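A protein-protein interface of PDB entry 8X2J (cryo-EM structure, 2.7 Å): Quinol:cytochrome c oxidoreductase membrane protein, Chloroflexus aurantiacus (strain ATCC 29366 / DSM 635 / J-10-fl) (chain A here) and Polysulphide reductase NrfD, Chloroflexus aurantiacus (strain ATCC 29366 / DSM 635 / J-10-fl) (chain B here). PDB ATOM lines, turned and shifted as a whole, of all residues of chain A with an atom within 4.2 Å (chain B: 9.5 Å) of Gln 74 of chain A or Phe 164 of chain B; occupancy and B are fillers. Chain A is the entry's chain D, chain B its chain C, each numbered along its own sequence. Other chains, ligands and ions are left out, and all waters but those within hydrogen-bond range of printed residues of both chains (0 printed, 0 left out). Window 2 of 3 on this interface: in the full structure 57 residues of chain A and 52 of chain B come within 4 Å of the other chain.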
ATOM      1  N   GLY A  70     -32.159  31.164  26.461  1.00  0.00           N
ATOM      2  CA  GLY A  70     -31.288  30.177  27.071  1.00  0.00           C
ATOM      3  C   GLY A  70     -31.420  30.104  28.576  1.00  0.00           C
ATOM      4  O   GLY A  70     -31.252  29.031  29.160  1.00  0.00           O
ATOM      5  N   PHE A  71     -31.704  31.233  29.232  1.00  0.00           N
ATOM      6  CA  PHE A  71     -31.977  31.167  30.664  1.00  0.00           C
ATOM      7  C   PHE A  71     -33.361  30.591  30.945  1.00  0.00           C
ATOM      8  O   PHE A  71     -33.518  29.769  31.857  1.00  0.00           O
ATOM      9  CB  PHE A  71     -31.832  32.545  31.302  1.00  0.00           C
ATOM     10  CG  PHE A  71     -31.536  32.493  32.773  1.00  0.00           C
ATOM     11  CD1 PHE A  71     -30.253  32.225  33.223  1.00  0.00           C
ATOM     12  CD2 PHE A  71     -32.543  32.690  33.703  1.00  0.00           C
ATOM     13  CE1 PHE A  71     -29.979  32.169  34.575  1.00  0.00           C
ATOM     14  CE2 PHE A  71     -32.276  32.633  35.055  1.00  0.00           C
ATOM     15  CZ  PHE A  71     -30.992  32.374  35.492  1.00  0.00           C
ATOM     16  N   ILE A  72     -34.371  31.007  30.174  1.00  0.00           N
ATOM     17  CA  ILE A  72     -35.752  30.596  30.411  1.00  0.00           C
ATOM     18  C   ILE A  72     -35.938  29.105  30.145  1.00  0.00           C
ATOM     19  O   ILE A  72     -36.655  28.426  30.891  1.00  0.00           O
ATOM     20  CB  ILE A  72     -36.699  31.479  29.565  1.00  0.00           C
ATOM     21  CG1 ILE A  72     -36.901  32.838  30.238  1.00  0.00           C
ATOM     22  CG2 ILE A  72     -38.054  30.831  29.318  1.00  0.00           C
ATOM     23  CD1 ILE A  72     -37.492  32.748  31.625  1.00  0.00           C
ATOM     24  N   LEU A  73     -35.262  28.566  29.125  1.00  0.00           N
ATOM     25  CA  LEU A  73     -35.372  27.146  28.804  1.00  0.00           C
ATOM     26  C   LEU A  73     -34.814  26.276  29.924  1.00  0.00           C
ATOM     27  O   LEU A  73     -35.465  25.320  30.360  1.00  0.00           O
ATOM     28  CB  LEU A  73     -34.648  26.861  27.488  1.00  0.00           C
ATOM     29  CG  LEU A  73     -34.574  25.411  27.015  1.00  0.00           C
ATOM     30  CD1 LEU A  73     -35.819  25.045  26.230  1.00  0.00           C
ATOM     31  CD2 LEU A  73     -33.324  25.197  26.184  1.00  0.00           C
ATOM     32  N   GLN A  74     -33.624  26.622  30.428  1.00  0.00           N
ATOM     33  CA  GLN A  74     -33.035  25.888  31.546  1.00  0.00           C
ATOM     34  C   GLN A  74     -33.858  26.040  32.815  1.00  0.00           C
ATOM     35  O   GLN A  74     -34.040  25.064  33.553  1.00  0.00           O
ATOM     36  CB  GLN A  74     -31.611  26.362  31.809  1.00  0.00           C
ATOM     37  CG  GLN A  74     -30.646  26.154  30.684  1.00  0.00           C
ATOM     38  CD  GLN A  74     -29.282  26.674  31.039  1.00  0.00           C
ATOM     39  OE1 GLN A  74     -28.449  25.947  31.578  1.00  0.00           O
ATOM     40  NE2 GLN A  74     -29.041  27.945  30.749  1.00  0.00           N
ATOM     41  N   TYR A  75     -34.369  27.252  33.076  1.00  0.00           N
ATOM     42  CA  TYR A  75     -35.161  27.501  34.276  1.00  0.00           C
ATOM     43  C   TYR A  75     -36.440  26.679  34.273  1.00  0.00           C
ATOM     44  O   TYR A  75     -36.710  25.944  35.229  1.00  0.00           O
ATOM     45  CB  TYR A  75     -35.485  28.992  34.391  1.00  0.00           C
ATOM     46  CG  TYR A  75     -35.807  29.442  35.799  1.00  0.00           C
ATOM     47  CD1 TYR A  75     -37.078  29.259  36.340  1.00  0.00           C
ATOM     48  CD2 TYR A  75     -34.843  30.053  36.585  1.00  0.00           C
ATOM     49  CE1 TYR A  75     -37.370  29.662  37.627  1.00  0.00           C
ATOM     50  CE2 TYR A  75     -35.127  30.457  37.872  1.00  0.00           C
ATOM     51  CZ  TYR A  75     -36.392  30.263  38.386  1.00  0.00           C
ATOM     52  OH  TYR A  75     -36.676  30.671  39.667  1.00  0.00           O
ATOM     53  N   ILE A  76     -37.212  26.760  33.185  1.00  0.00           N
ATOM     54  CA  ILE A  76     -38.469  26.025  33.077  1.00  0.00           C
ATOM     55  C   ILE A  76     -38.210  24.525  33.102  1.00  0.00           C
ATOM     56  O   ILE A  76     -38.840  23.790  33.873  1.00  0.00           O
ATOM     57  CB  ILE A  76     -39.230  26.451  31.807  1.00  0.00           C
ATOM     58  CG1 ILE A  76     -39.722  27.895  31.929  1.00  0.00           C
ATOM     59  CG2 ILE A  76     -40.405  25.522  31.537  1.00  0.00           C
ATOM     60  CD1 ILE A  76     -40.749  28.114  33.015  1.00  0.00           C
ATOM     61  N   GLY A  77     -37.215  24.067  32.337  1.00  0.00           N
ATOM     62  CA  GLY A  77     -36.981  22.640  32.209  1.00  0.00           C
ATOM     63  C   GLY A  77     -36.457  21.972  33.464  1.00  0.00           C
ATOM     64  O   GLY A  77     -36.879  20.865  33.803  1.00  0.00           O
ATOM     65  N   ASN A  78     -35.552  22.627  34.183  1.00  0.00           N
ATOM     66  CA  ASN A  78     -34.994  22.009  35.373  1.00  0.00           C
ATOM     67  C   ASN A  78     -35.731  22.378  36.642  1.00  0.00           C
ATOM     68  O   ASN A  78     -35.506  21.738  37.676  1.00  0.00           O
ATOM     69  CB  ASN A  78     -33.532  22.404  35.549  1.00  0.00           C
ATOM     70  CG  ASN A  78     -32.676  21.924  34.427  1.00  0.00           C
ATOM     71  OD1 ASN A  78     -32.023  22.713  33.761  1.00  0.00           O
ATOM     72  ND2 ASN A  78     -32.669  20.617  34.201  1.00  0.00           N
ATOM     73  N   ALA A  98     -24.355  27.182  36.520  1.00  0.00           N
ATOM     74  CA  ALA A  98     -24.773  26.112  35.605  1.00  0.00           C
ATOM     75  C   ALA A  98     -26.041  26.480  34.837  1.00  0.00           C
ATOM     76  O   ALA A  98     -26.840  25.611  34.485  1.00  0.00           O
ATOM     77  CB  ALA A  98     -24.943  24.762  36.317  1.00  0.00           C
ATOM     78  N   MET A  99     -26.237  27.775  34.581  1.00  0.00           N
ATOM     79  CA  MET A  99     -27.245  28.265  33.649  1.00  0.00           C
ATOM     80  C   MET A  99     -26.584  29.291  32.738  1.00  0.00           C
ATOM     81  O   MET A  99     -27.013  29.516  31.596  1.00  0.00           O
ATOM     82  CB  MET A  99     -28.433  28.875  34.394  1.00  0.00           C
ATOM     83  CG  MET A  99     -29.253  27.877  35.192  1.00  0.00           C
ATOM     84  SD  MET A  99     -30.704  28.607  35.965  1.00  0.00           S
ATOM     85  CE  MET A  99     -31.704  28.933  34.525  1.00  0.00           C
ATOM     86  N   ILE A 102     -25.035  27.786  29.031  1.00  0.00           N
ATOM     87  CA  ILE A 102     -26.019  27.575  27.974  1.00  0.00           C
ATOM     88  C   ILE A 102     -26.735  28.882  27.626  1.00  0.00           C
ATOM     89  O   ILE A 102     -27.048  29.129  26.449  1.00  0.00           O
ATOM     90  CB  ILE A 102     -26.969  26.439  28.402  1.00  0.00           C
ATOM     91  CG1 ILE A 102     -26.236  25.106  28.289  1.00  0.00           C
ATOM     92  CG2 ILE A 102     -28.248  26.394  27.579  1.00  0.00           C
ATOM     93  CD1 ILE A 102     -26.833  24.021  29.107  1.00  0.00           C
ATOM     94  N   THR A 103     -26.936  29.760  28.621  1.00  0.00           N
ATOM     95  CA  THR A 103     -27.459  31.104  28.371  1.00  0.00           C
ATOM     96  C   THR A 103     -26.551  31.891  27.427  1.00  0.00           C
ATOM     97  O   THR A 103     -27.010  32.470  26.429  1.00  0.00           O
ATOM     98  CB  THR A 103     -27.603  31.843  29.704  1.00  0.00           C
ATOM     99  OG1 THR A 103     -28.643  31.240  30.482  1.00  0.00           O
ATOM    100  CG2 THR A 103     -27.921  33.312  29.494  1.00  0.00           C
ATOM    101  N   TYR B 149     -29.112  12.767  20.727  1.00  0.00           N
ATOM    102  CA  TYR B 149     -30.148  13.788  20.731  1.00  0.00           C
ATOM    103  C   TYR B 149     -30.890  13.882  22.056  1.00  0.00           C
ATOM    104  O   TYR B 149     -31.686  14.809  22.232  1.00  0.00           O
ATOM    105  CB  TYR B 149     -31.141  13.534  19.590  1.00  0.00           C
ATOM    106  CG  TYR B 149     -32.011  12.302  19.742  1.00  0.00           C
ATOM    107  CD1 TYR B 149     -31.504  11.027  19.513  1.00  0.00           C
ATOM    108  CD2 TYR B 149     -33.349  12.418  20.082  1.00  0.00           C
ATOM    109  CE1 TYR B 149     -32.298   9.909  19.648  1.00  0.00           C
ATOM    110  CE2 TYR B 149     -34.150  11.306  20.211  1.00  0.00           C
ATOM    111  CZ  TYR B 149     -33.618  10.055  19.996  1.00  0.00           C
ATOM    112  OH  TYR B 149     -34.413   8.943  20.124  1.00  0.00           O
ATOM    113  N   TRP B 150     -30.662  12.949  22.982  1.00  0.00           N
ATOM    114  CA  TRP B 150     -31.251  13.077  24.309  1.00  0.00           C
ATOM    115  C   TRP B 150     -30.491  14.093  25.151  1.00  0.00           C
ATOM    116  O   TRP B 150     -31.030  14.612  26.135  1.00  0.00           O
ATOM    117  CB  TRP B 150     -31.295  11.713  24.998  1.00  0.00           C
ATOM    118  CG  TRP B 150     -32.415  10.867  24.490  1.00  0.00           C
ATOM    119  CD1 TRP B 150     -33.326  11.220  23.551  1.00  0.00           C
ATOM    120  CD2 TRP B 150     -32.749   9.531  24.888  1.00  0.00           C
ATOM    121  NE1 TRP B 150     -34.209  10.198  23.333  1.00  0.00           N
ATOM    122  CE2 TRP B 150     -33.876   9.147  24.142  1.00  0.00           C
ATOM    123  CE3 TRP B 150     -32.205   8.624  25.801  1.00  0.00           C
ATOM    124  CZ2 TRP B 150     -34.471   7.899  24.279  1.00  0.00           C
ATOM    125  CZ3 TRP B 150     -32.800   7.385  25.930  1.00  0.00           C
ATOM    126  CH2 TRP B 150     -33.917   7.034  25.174  1.00  0.00           C
ATOM    127  N   LEU B 151     -29.246  14.385  24.778  1.00  0.00           N
ATOM    128  CA  LEU B 151     -28.494  15.463  25.404  1.00  0.00           C
ATOM    129  C   LEU B 151     -28.952  16.828  24.908  1.00  0.00           C
ATOM    130  O   LEU B 151     -28.796  17.826  25.618  1.00  0.00           O
ATOM    131  CB  LEU B 151     -27.000  15.286  25.137  1.00  0.00           C
ATOM    132  CG  LEU B 151     -26.199  14.277  25.960  1.00  0.00           C
ATOM    133  CD1 LEU B 151     -26.299  12.875  25.388  1.00  0.00           C
ATOM    134  CD2 LEU B 151     -24.757  14.713  26.029  1.00  0.00           C
ATOM    135  N   ILE B 152     -29.488  16.890  23.696  1.00  0.00           N
ATOM    136  CA  ILE B 152     -30.055  18.105  23.120  1.00  0.00           C
ATOM    137  C   ILE B 152     -31.428  18.332  23.741  1.00  0.00           C
ATOM    138  O   ILE B 152     -32.185  17.366  23.915  1.00  0.00           O
ATOM    139  CB  ILE B 152     -30.137  17.996  21.586  1.00  0.00           C
ATOM    140  CG1 ILE B 152     -28.776  17.614  21.004  1.00  0.00           C
ATOM    141  CG2 ILE B 152     -30.639  19.286  20.953  1.00  0.00           C
ATOM    142  CD1 ILE B 152     -28.843  17.130  19.577  1.00  0.00           C
ATOM    143  N   PRO B 153     -31.793  19.568  24.110  1.00  0.00           N
ATOM    144  CA  PRO B 153     -33.179  19.820  24.525  1.00  0.00           C
ATOM    145  C   PRO B 153     -34.137  19.757  23.348  1.00  0.00           C
ATOM    146  O   PRO B 153     -34.228  20.693  22.549  1.00  0.00           O
ATOM    147  CB  PRO B 153     -33.122  21.230  25.128  1.00  0.00           C
ATOM    148  CG  PRO B 153     -31.886  21.842  24.568  1.00  0.00           C
ATOM    149  CD  PRO B 153     -30.918  20.723  24.367  1.00  0.00           C
ATOM    150  N   TYR B 154     -34.869  18.656  23.246  1.00  0.00           N
ATOM    151  CA  TYR B 154     -35.797  18.402  22.159  1.00  0.00           C
ATOM    152  C   TYR B 154     -37.129  17.960  22.742  1.00  0.00           C
ATOM    153  O   TYR B 154     -37.168  17.380  23.831  1.00  0.00           O
ATOM    154  CB  TYR B 154     -35.245  17.327  21.204  1.00  0.00           C
ATOM    155  CG  TYR B 154     -35.519  15.906  21.635  1.00  0.00           C
ATOM    156  CD1 TYR B 154     -34.873  15.359  22.734  1.00  0.00           C
ATOM    157  CD2 TYR B 154     -36.430  15.115  20.948  1.00  0.00           C
ATOM    158  CE1 TYR B 154     -35.127  14.070  23.136  1.00  0.00           C
ATOM    159  CE2 TYR B 154     -36.688  13.821  21.343  1.00  0.00           C
ATOM    160  CZ  TYR B 154     -36.033  13.306  22.436  1.00  0.00           C
ATOM    161  OH  TYR B 154     -36.287  12.017  22.834  1.00  0.00           O
ATOM    162  N   MET B 160     -39.102  14.427  29.320  1.00  0.00           N
ATOM    163  CA  MET B 160     -37.750  14.461  29.853  1.00  0.00           C
ATOM    164  C   MET B 160     -37.008  15.699  29.371  1.00  0.00           C
ATOM    165  O   MET B 160     -37.312  16.270  28.321  1.00  0.00           O
ATOM    166  CB  MET B 160     -36.981  13.209  29.436  1.00  0.00           C
ATOM    167  CG  MET B 160     -37.001  12.082  30.446  1.00  0.00           C
ATOM    168  SD  MET B 160     -36.775  12.619  32.150  1.00  0.00           S
ATOM    169  CE  MET B 160     -35.031  13.008  32.162  1.00  0.00           C
ATOM    170  N   TRP B 161     -36.018  16.105  30.153  1.00  0.00           N
ATOM    171  CA  TRP B 161     -35.137  17.219  29.854  1.00  0.00           C
ATOM    172  C   TRP B 161     -33.695  16.788  30.059  1.00  0.00           C
ATOM    173  O   TRP B 161     -33.427  15.859  30.826  1.00  0.00           O
ATOM    174  CB  TRP B 161     -35.430  18.423  30.761  1.00  0.00           C
ATOM    175  CG  TRP B 161     -36.750  19.070  30.538  1.00  0.00           C
ATOM    176  CD1 TRP B 161     -37.949  18.676  31.046  1.00  0.00           C
ATOM    177  CD2 TRP B 161     -37.008  20.237  29.755  1.00  0.00           C
ATOM    178  NE1 TRP B 161     -38.941  19.525  30.628  1.00  0.00           N
ATOM    179  CE2 TRP B 161     -38.388  20.495  29.835  1.00  0.00           C
ATOM    180  CE3 TRP B 161     -36.202  21.097  29.004  1.00  0.00           C
ATOM    181  CZ2 TRP B 161     -38.983  21.572  29.186  1.00  0.00           C
ATOM    182  CZ3 TRP B 161     -36.795  22.164  28.360  1.00  0.00           C
ATOM    183  CH2 TRP B 161     -38.173  22.392  28.455  1.00  0.00           C
ATOM    184  N   PRO B 162     -32.747  17.430  29.381  1.00  0.00           N
ATOM    185  CA  PRO B 162     -31.354  17.334  29.821  1.00  0.00           C
ATOM    186  C   PRO B 162     -31.185  18.055  31.147  1.00  0.00           C
ATOM    187  O   PRO B 162     -31.970  18.939  31.497  1.00  0.00           O
ATOM    188  CB  PRO B 162     -30.569  18.023  28.700  1.00  0.00           C
ATOM    189  CG  PRO B 162     -31.507  18.102  27.551  1.00  0.00           C
ATOM    190  CD  PRO B 162     -32.873  18.190  28.127  1.00  0.00           C
ATOM    191  N   GLN B 163     -30.159  17.646  31.900  1.00  0.00           N
ATOM    192  CA  GLN B 163     -29.993  18.152  33.259  1.00  0.00           C
ATOM    193  C   GLN B 163     -29.633  19.633  33.274  1.00  0.00           C
ATOM    194  O   GLN B 163     -30.098  20.376  34.147  1.00  0.00           O
ATOM    195  CB  GLN B 163     -28.918  17.360  33.998  1.00  0.00           C
ATOM    196  CG  GLN B 163     -28.747  17.787  35.444  1.00  0.00           C
ATOM    197  CD  GLN B 163     -27.458  17.322  36.054  1.00  0.00           C
ATOM    198  OE1 GLN B 163     -27.157  17.640  37.199  1.00  0.00           O
ATOM    199  NE2 GLN B 163     -26.669  16.594  35.287  1.00  0.00           N
ATOM    200  N   PHE B 164     -28.755  20.061  32.361  1.00  0.00           N
ATOM    201  CA  PHE B 164     -28.221  21.414  32.169  1.00  0.00           C
ATOM    202  C   PHE B 164     -27.326  21.881  33.318  1.00  0.00           C
ATOM    203  O   PHE B 164     -26.742  22.962  33.220  1.00  0.00           O
ATOM    204  CB  PHE B 164     -29.313  22.473  31.935  1.00  0.00           C
ATOM    205  CG  PHE B 164     -30.126  22.261  30.688  1.00  0.00           C
ATOM    206  CD1 PHE B 164     -29.547  21.753  29.539  1.00  0.00           C
ATOM    207  CD2 PHE B 164     -31.472  22.582  30.666  1.00  0.00           C
ATOM    208  CE1 PHE B 164     -30.297  21.579  28.393  1.00  0.00           C
ATOM    209  CE2 PHE B 164     -32.229  22.399  29.530  1.00  0.00           C
ATOM    210  CZ  PHE B 164     -31.640  21.898  28.393  1.00  0.00           C
ATOM    211  N   ARG B 165     -27.195  21.109  34.396  1.00  0.00           N
ATOM    212  CA  ARG B 165     -26.234  21.371  35.457  1.00  0.00           C
ATOM    213  C   ARG B 165     -24.908  20.685  35.193  1.00  0.00           C
ATOM    214  O   ARG B 165     -23.870  21.130  35.695  1.00  0.00           O
ATOM    215  CB  ARG B 165     -26.792  20.909  36.809  1.00  0.00           C
ATOM    216  CG  ARG B 165     -27.537  21.968  37.608  1.00  0.00           C
ATOM    217  CD  ARG B 165     -28.878  22.366  36.998  1.00  0.00           C
ATOM    218  NE  ARG B 165     -29.797  21.256  36.773  1.00  0.00           N
ATOM    219  CZ  ARG B 165     -30.661  20.800  37.670  1.00  0.00           C
ATOM    220  NH1 ARG B 165     -30.694  21.279  38.902  1.00  0.00           N
ATOM    221  NH2 ARG B 165     -31.524  19.853  37.315  1.00  0.00           N
ATOM    222  N   SER B 166     -24.931  19.605  34.422  1.00  0.00           N
ATOM    223  CA  SER B 166     -23.717  18.957  33.972  1.00  0.00           C
ATOM    224  C   SER B 166     -23.026  19.810  32.922  1.00  0.00           C
ATOM    225  O   SER B 166     -23.646  20.623  32.234  1.00  0.00           O
ATOM    226  CB  SER B 166     -24.028  17.596  33.370  1.00  0.00           C
ATOM    227  OG  SER B 166     -24.513  17.783  32.059  1.00  0.00           O
ATOM    228  N   ALA B 167     -21.725  19.594  32.781  1.00  0.00           N
ATOM    229  CA  ALA B 167     -20.976  20.329  31.780  1.00  0.00           C
ATOM    230  C   ALA B 167     -21.093  19.726  30.389  1.00  0.00           C
ATOM    231  O   ALA B 167     -20.708  20.379  29.420  1.00  0.00           O
ATOM    232  CB  ALA B 167     -19.514  20.419  32.191  1.00  0.00           C
ATOM    233  N   LEU B 168     -21.638  18.518  30.254  1.00  0.00           N
ATOM    234  CA  LEU B 168     -21.795  17.942  28.925  1.00  0.00           C
ATOM    235  C   LEU B 168     -22.978  18.542  28.173  1.00  0.00           C
ATOM    236  O   LEU B 168     -22.963  18.576  26.940  1.00  0.00           O
ATOM    237  CB  LEU B 168     -21.928  16.424  29.019  1.00  0.00           C
ATOM    238  CG  LEU B 168     -20.807  15.671  29.740  1.00  0.00           C
ATOM    239  CD1 LEU B 168     -20.969  14.173  29.556  1.00  0.00           C
ATOM    240  CD2 LEU B 168     -19.438  16.122  29.272  1.00  0.00           C
ATOM    241  N   ALA B 169     -23.997  19.039  28.879  1.00  0.00           N
ATOM    242  CA  ALA B 169     -25.041  19.815  28.211  1.00  0.00           C
ATOM    243  C   ALA B 169     -24.500  21.156  27.721  1.00  0.00           C
ATOM    244  O   ALA B 169     -24.845  21.617  26.618  1.00  0.00           O
ATOM    245  CB  ALA B 169     -26.225  20.018  29.153  1.00  0.00           C
ATOM    246  N   TRP B 170     -23.635  21.783  28.525  1.00  0.00           N
ATOM    247  CA  TRP B 170     -22.929  22.980  28.084  1.00  0.00           C
ATOM    248  C   TRP B 170     -22.026  22.659  26.903  1.00  0.00           C
ATOM    249  O   TRP B 170     -21.824  23.498  26.026  1.00  0.00           O
ATOM    250  CB  TRP B 170     -22.076  23.587  29.206  1.00  0.00           C
ATOM    251  CG  TRP B 170     -22.601  23.625  30.620  1.00  0.00           C
ATOM    252  CD1 TRP B 170     -23.898  23.551  31.044  1.00  0.00           C
ATOM    253  CD2 TRP B 170     -21.807  23.775  31.798  1.00  0.00           C
ATOM    254  NE1 TRP B 170     -23.952  23.628  32.411  1.00  0.00           N
ATOM    255  CE2 TRP B 170     -22.680  23.770  32.897  1.00  0.00           C
ATOM    256  CE3 TRP B 170     -20.435  23.911  32.028  1.00  0.00           C
ATOM    257  CZ2 TRP B 170     -22.226  23.889  34.205  1.00  0.00           C
ATOM    258  CZ3 TRP B 170     -19.991  24.026  33.328  1.00  0.00           C
ATOM    259  CH2 TRP B 170     -20.884  24.019  34.399  1.00  0.00           C
ATOM    260  N   ASP B 171     -21.461  21.450  26.883  1.00  0.00           N
ATOM    261  CA  ASP B 171     -20.665  20.992  25.750  1.00  0.00           C
ATOM    262  C   ASP B 171     -21.508  20.822  24.495  1.00  0.00           C
ATOM    263  O   ASP B 171     -21.030  21.102  23.393  1.00  0.00           O
ATOM    264  CB  ASP B 171     -19.975  19.682  26.101  1.00  0.00           C
ATOM    265  CG  ASP B 171     -18.871  19.863  27.099  1.00  0.00           C
ATOM    266  OD1 ASP B 171     -18.447  21.012  27.310  1.00  0.00           O
ATOM    267  OD2 ASP B 171     -18.437  18.855  27.684  1.00  0.00           O
ATOM    268  N   VAL B 172     -22.745  20.332  24.643  1.00  0.00           N
ATOM    269  CA  VAL B 172     -23.675  20.244  23.512  1.00  0.00           C
ATOM    270  C   VAL B 172     -23.907  21.624  22.915  1.00  0.00           C
ATOM    271  O   VAL B 172     -23.715  21.842  21.708  1.00  0.00           O
ATOM    272  CB  VAL B 172     -25.012  19.617  23.950  1.00  0.00           C
ATOM    273  CG1 VAL B 172     -26.067  19.784  22.863  1.00  0.00           C
ATOM    274  CG2 VAL B 172     -24.853  18.173  24.289  1.00  0.00           C
ATOM    275  N   PHE B 173     -24.262  22.585  23.775  1.00  0.00           N
ATOM    276  CA  PHE B 173     -24.539  23.943  23.310  1.00  0.00           C
ATOM    277  C   PHE B 173     -23.289  24.619  22.757  1.00  0.00           C
ATOM    278  O   PHE B 173     -23.347  25.284  21.718  1.00  0.00           O
ATOM    279  CB  PHE B 173     -25.147  24.767  24.441  1.00  0.00           C
ATOM    280  CG  PHE B 173     -26.643  24.714  24.483  1.00  0.00           C
ATOM    281  CD1 PHE B 173     -27.292  23.645  25.077  1.00  0.00           C
ATOM    282  CD2 PHE B 173     -27.400  25.726  23.919  1.00  0.00           C
ATOM    283  CE1 PHE B 173     -28.670  23.592  25.115  1.00  0.00           C
ATOM    284  CE2 PHE B 173     -28.778  25.678  23.954  1.00  0.00           C
ATOM    285  CZ  PHE B 173     -29.413  24.609  24.552  1.00  0.00           C
ATOM    286  N   ILE B 255     -15.663  20.563  36.713  1.00  0.00           N
ATOM    287  CA  ILE B 255     -16.822  20.510  37.604  1.00  0.00           C
ATOM    288  C   ILE B 255     -16.880  19.218  38.399  1.00  0.00           C
ATOM    289  O   ILE B 255     -17.739  19.076  39.275  1.00  0.00           O
ATOM    290  CB  ILE B 255     -18.171  20.655  36.874  1.00  0.00           C
ATOM    291  CG1 ILE B 255     -18.456  19.445  35.984  1.00  0.00           C
ATOM    292  CG2 ILE B 255     -18.236  21.955  36.098  1.00  0.00           C
ATOM    293  CD1 ILE B 255     -19.929  19.195  35.758  1.00  0.00           C
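The guanidinium group of Arg 165 of chain B sits at hydrogen-bond distance from the backbone carbonyl oxygen of Gln 163 of chain B (2.8 Å).
O of Phe 164 of chain B is in hydrogen-bond range of NE1 of Trp 170 of chain B (3.0 Å).
The side-chain hydroxyl of Ser 166 of chain B sits at hydrogen-bond distance from the backbone NH of Ala 169 of chain B (3.5 Å).
O of Gln 74 of chain A sits close to OD1 of Asn 78 of chain A, 3.1 Å away.
O of Ala 98 of chain A sits close to OE1 of Gln 74 of chain A (3.3 Å).
The side-chain hydroxyl of Thr 103 of chain A sits at hydrogen-bond distance from the side-chain amide nitrogen of Gln 74 of chain A (3.3 Å).
Printed residues of chain B within 4 Å of Gln 74 of chain A: Phe 164 (3.6 Å).
Phe 164 of chain B touches just these residues of chain A: Gln 74 (3.6 Å), Asn 78 (3.1 Å), Ala 98 (2.9 Å) and Ile 102 (3.6 Å).
Gly 77 of chain A touches one residue of chain B.
No residue of chain B comes within 4 Å of Met 99 of chain A.
Ile 102 of chain A touches four residues of chain B.
Of the printed residues of chain A, Phe 173 of chain B touches Ile 102.
Of the printed residues of chain B, Leu 73 of chain A touches Pro 153 (3.99 Å) and Trp 161 (3.7 Å).
Printed residues of chain A within 4 Å of Gln 163 of chain B: Asn 78 (2.6 Å).
Of the printed residues of chain B, Ala 98 of chain A touches Phe 164, Arg 165 and Trp 170.
Val 172 of chain B touches none of the printed residues of chain A.
The nearest printed residue of chain A that does not touch Phe 164 of chain B is Leu 73 of chain A (4.3 Å).
The nearest printed residue of chain A that does not touch Phe 173 of chain B is Leu 73 of chain A (4.3 Å).
Of the 13 printed residues of chain A, 6 touch a printed residue of chain B.
Hydrophobic or aromatic side chains of chain B that line the printed part of chain A: Pro 153, Trp 161, Phe 164, Trp 170 and Phe 173.
Among the printed residues, no Asp or Glu carboxylate lies within 4 Å of a Lys or Arg side-chain nitrogen of the other chain.
The backbone carbonyl oxygen of Pro 162 of chain B is in hydrogen-bond range of the side-chain amide nitrogen of Asn 78 of chain A (3.3 Å).
The backbone carbonyl oxygen of Gln 163 of chain B lies within hydrogen-bond range of the side-chain amide nitrogen of Asn 78 of chain A.
The side-chain amide nitrogen of Asn 78 of chain A lies close to the guanidinium group of Arg 165 of chain B, at 3.4 Å.
O of Ala 98 of chain A lies close to O of Phe 164 of chain B, 2.9 Å away.
Among the printed residues, merely in contact across the chains: Asn 78 of chain A with Phe 164 of chain B, Gly 77 of chain A with Trp 161 of chain B, Ile 102 of chain A with Trp 170 of chain B, Ala 98 of chain A with Trp 170 of chain B, Ile 102 of chain A with Phe 164 of chain B, Gln 74 of chain A with Phe 164 of chain B, Ile 102 of chain A with Phe 173 of chain B, Leu 73 of chain A with Trp 161 of chain B, Ala 98 of chain A with Arg 165 of chain B, Ile 102 of chain A with Ala 169 of chain B and Leu 73 of chain A with Pro 153 of chain B.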
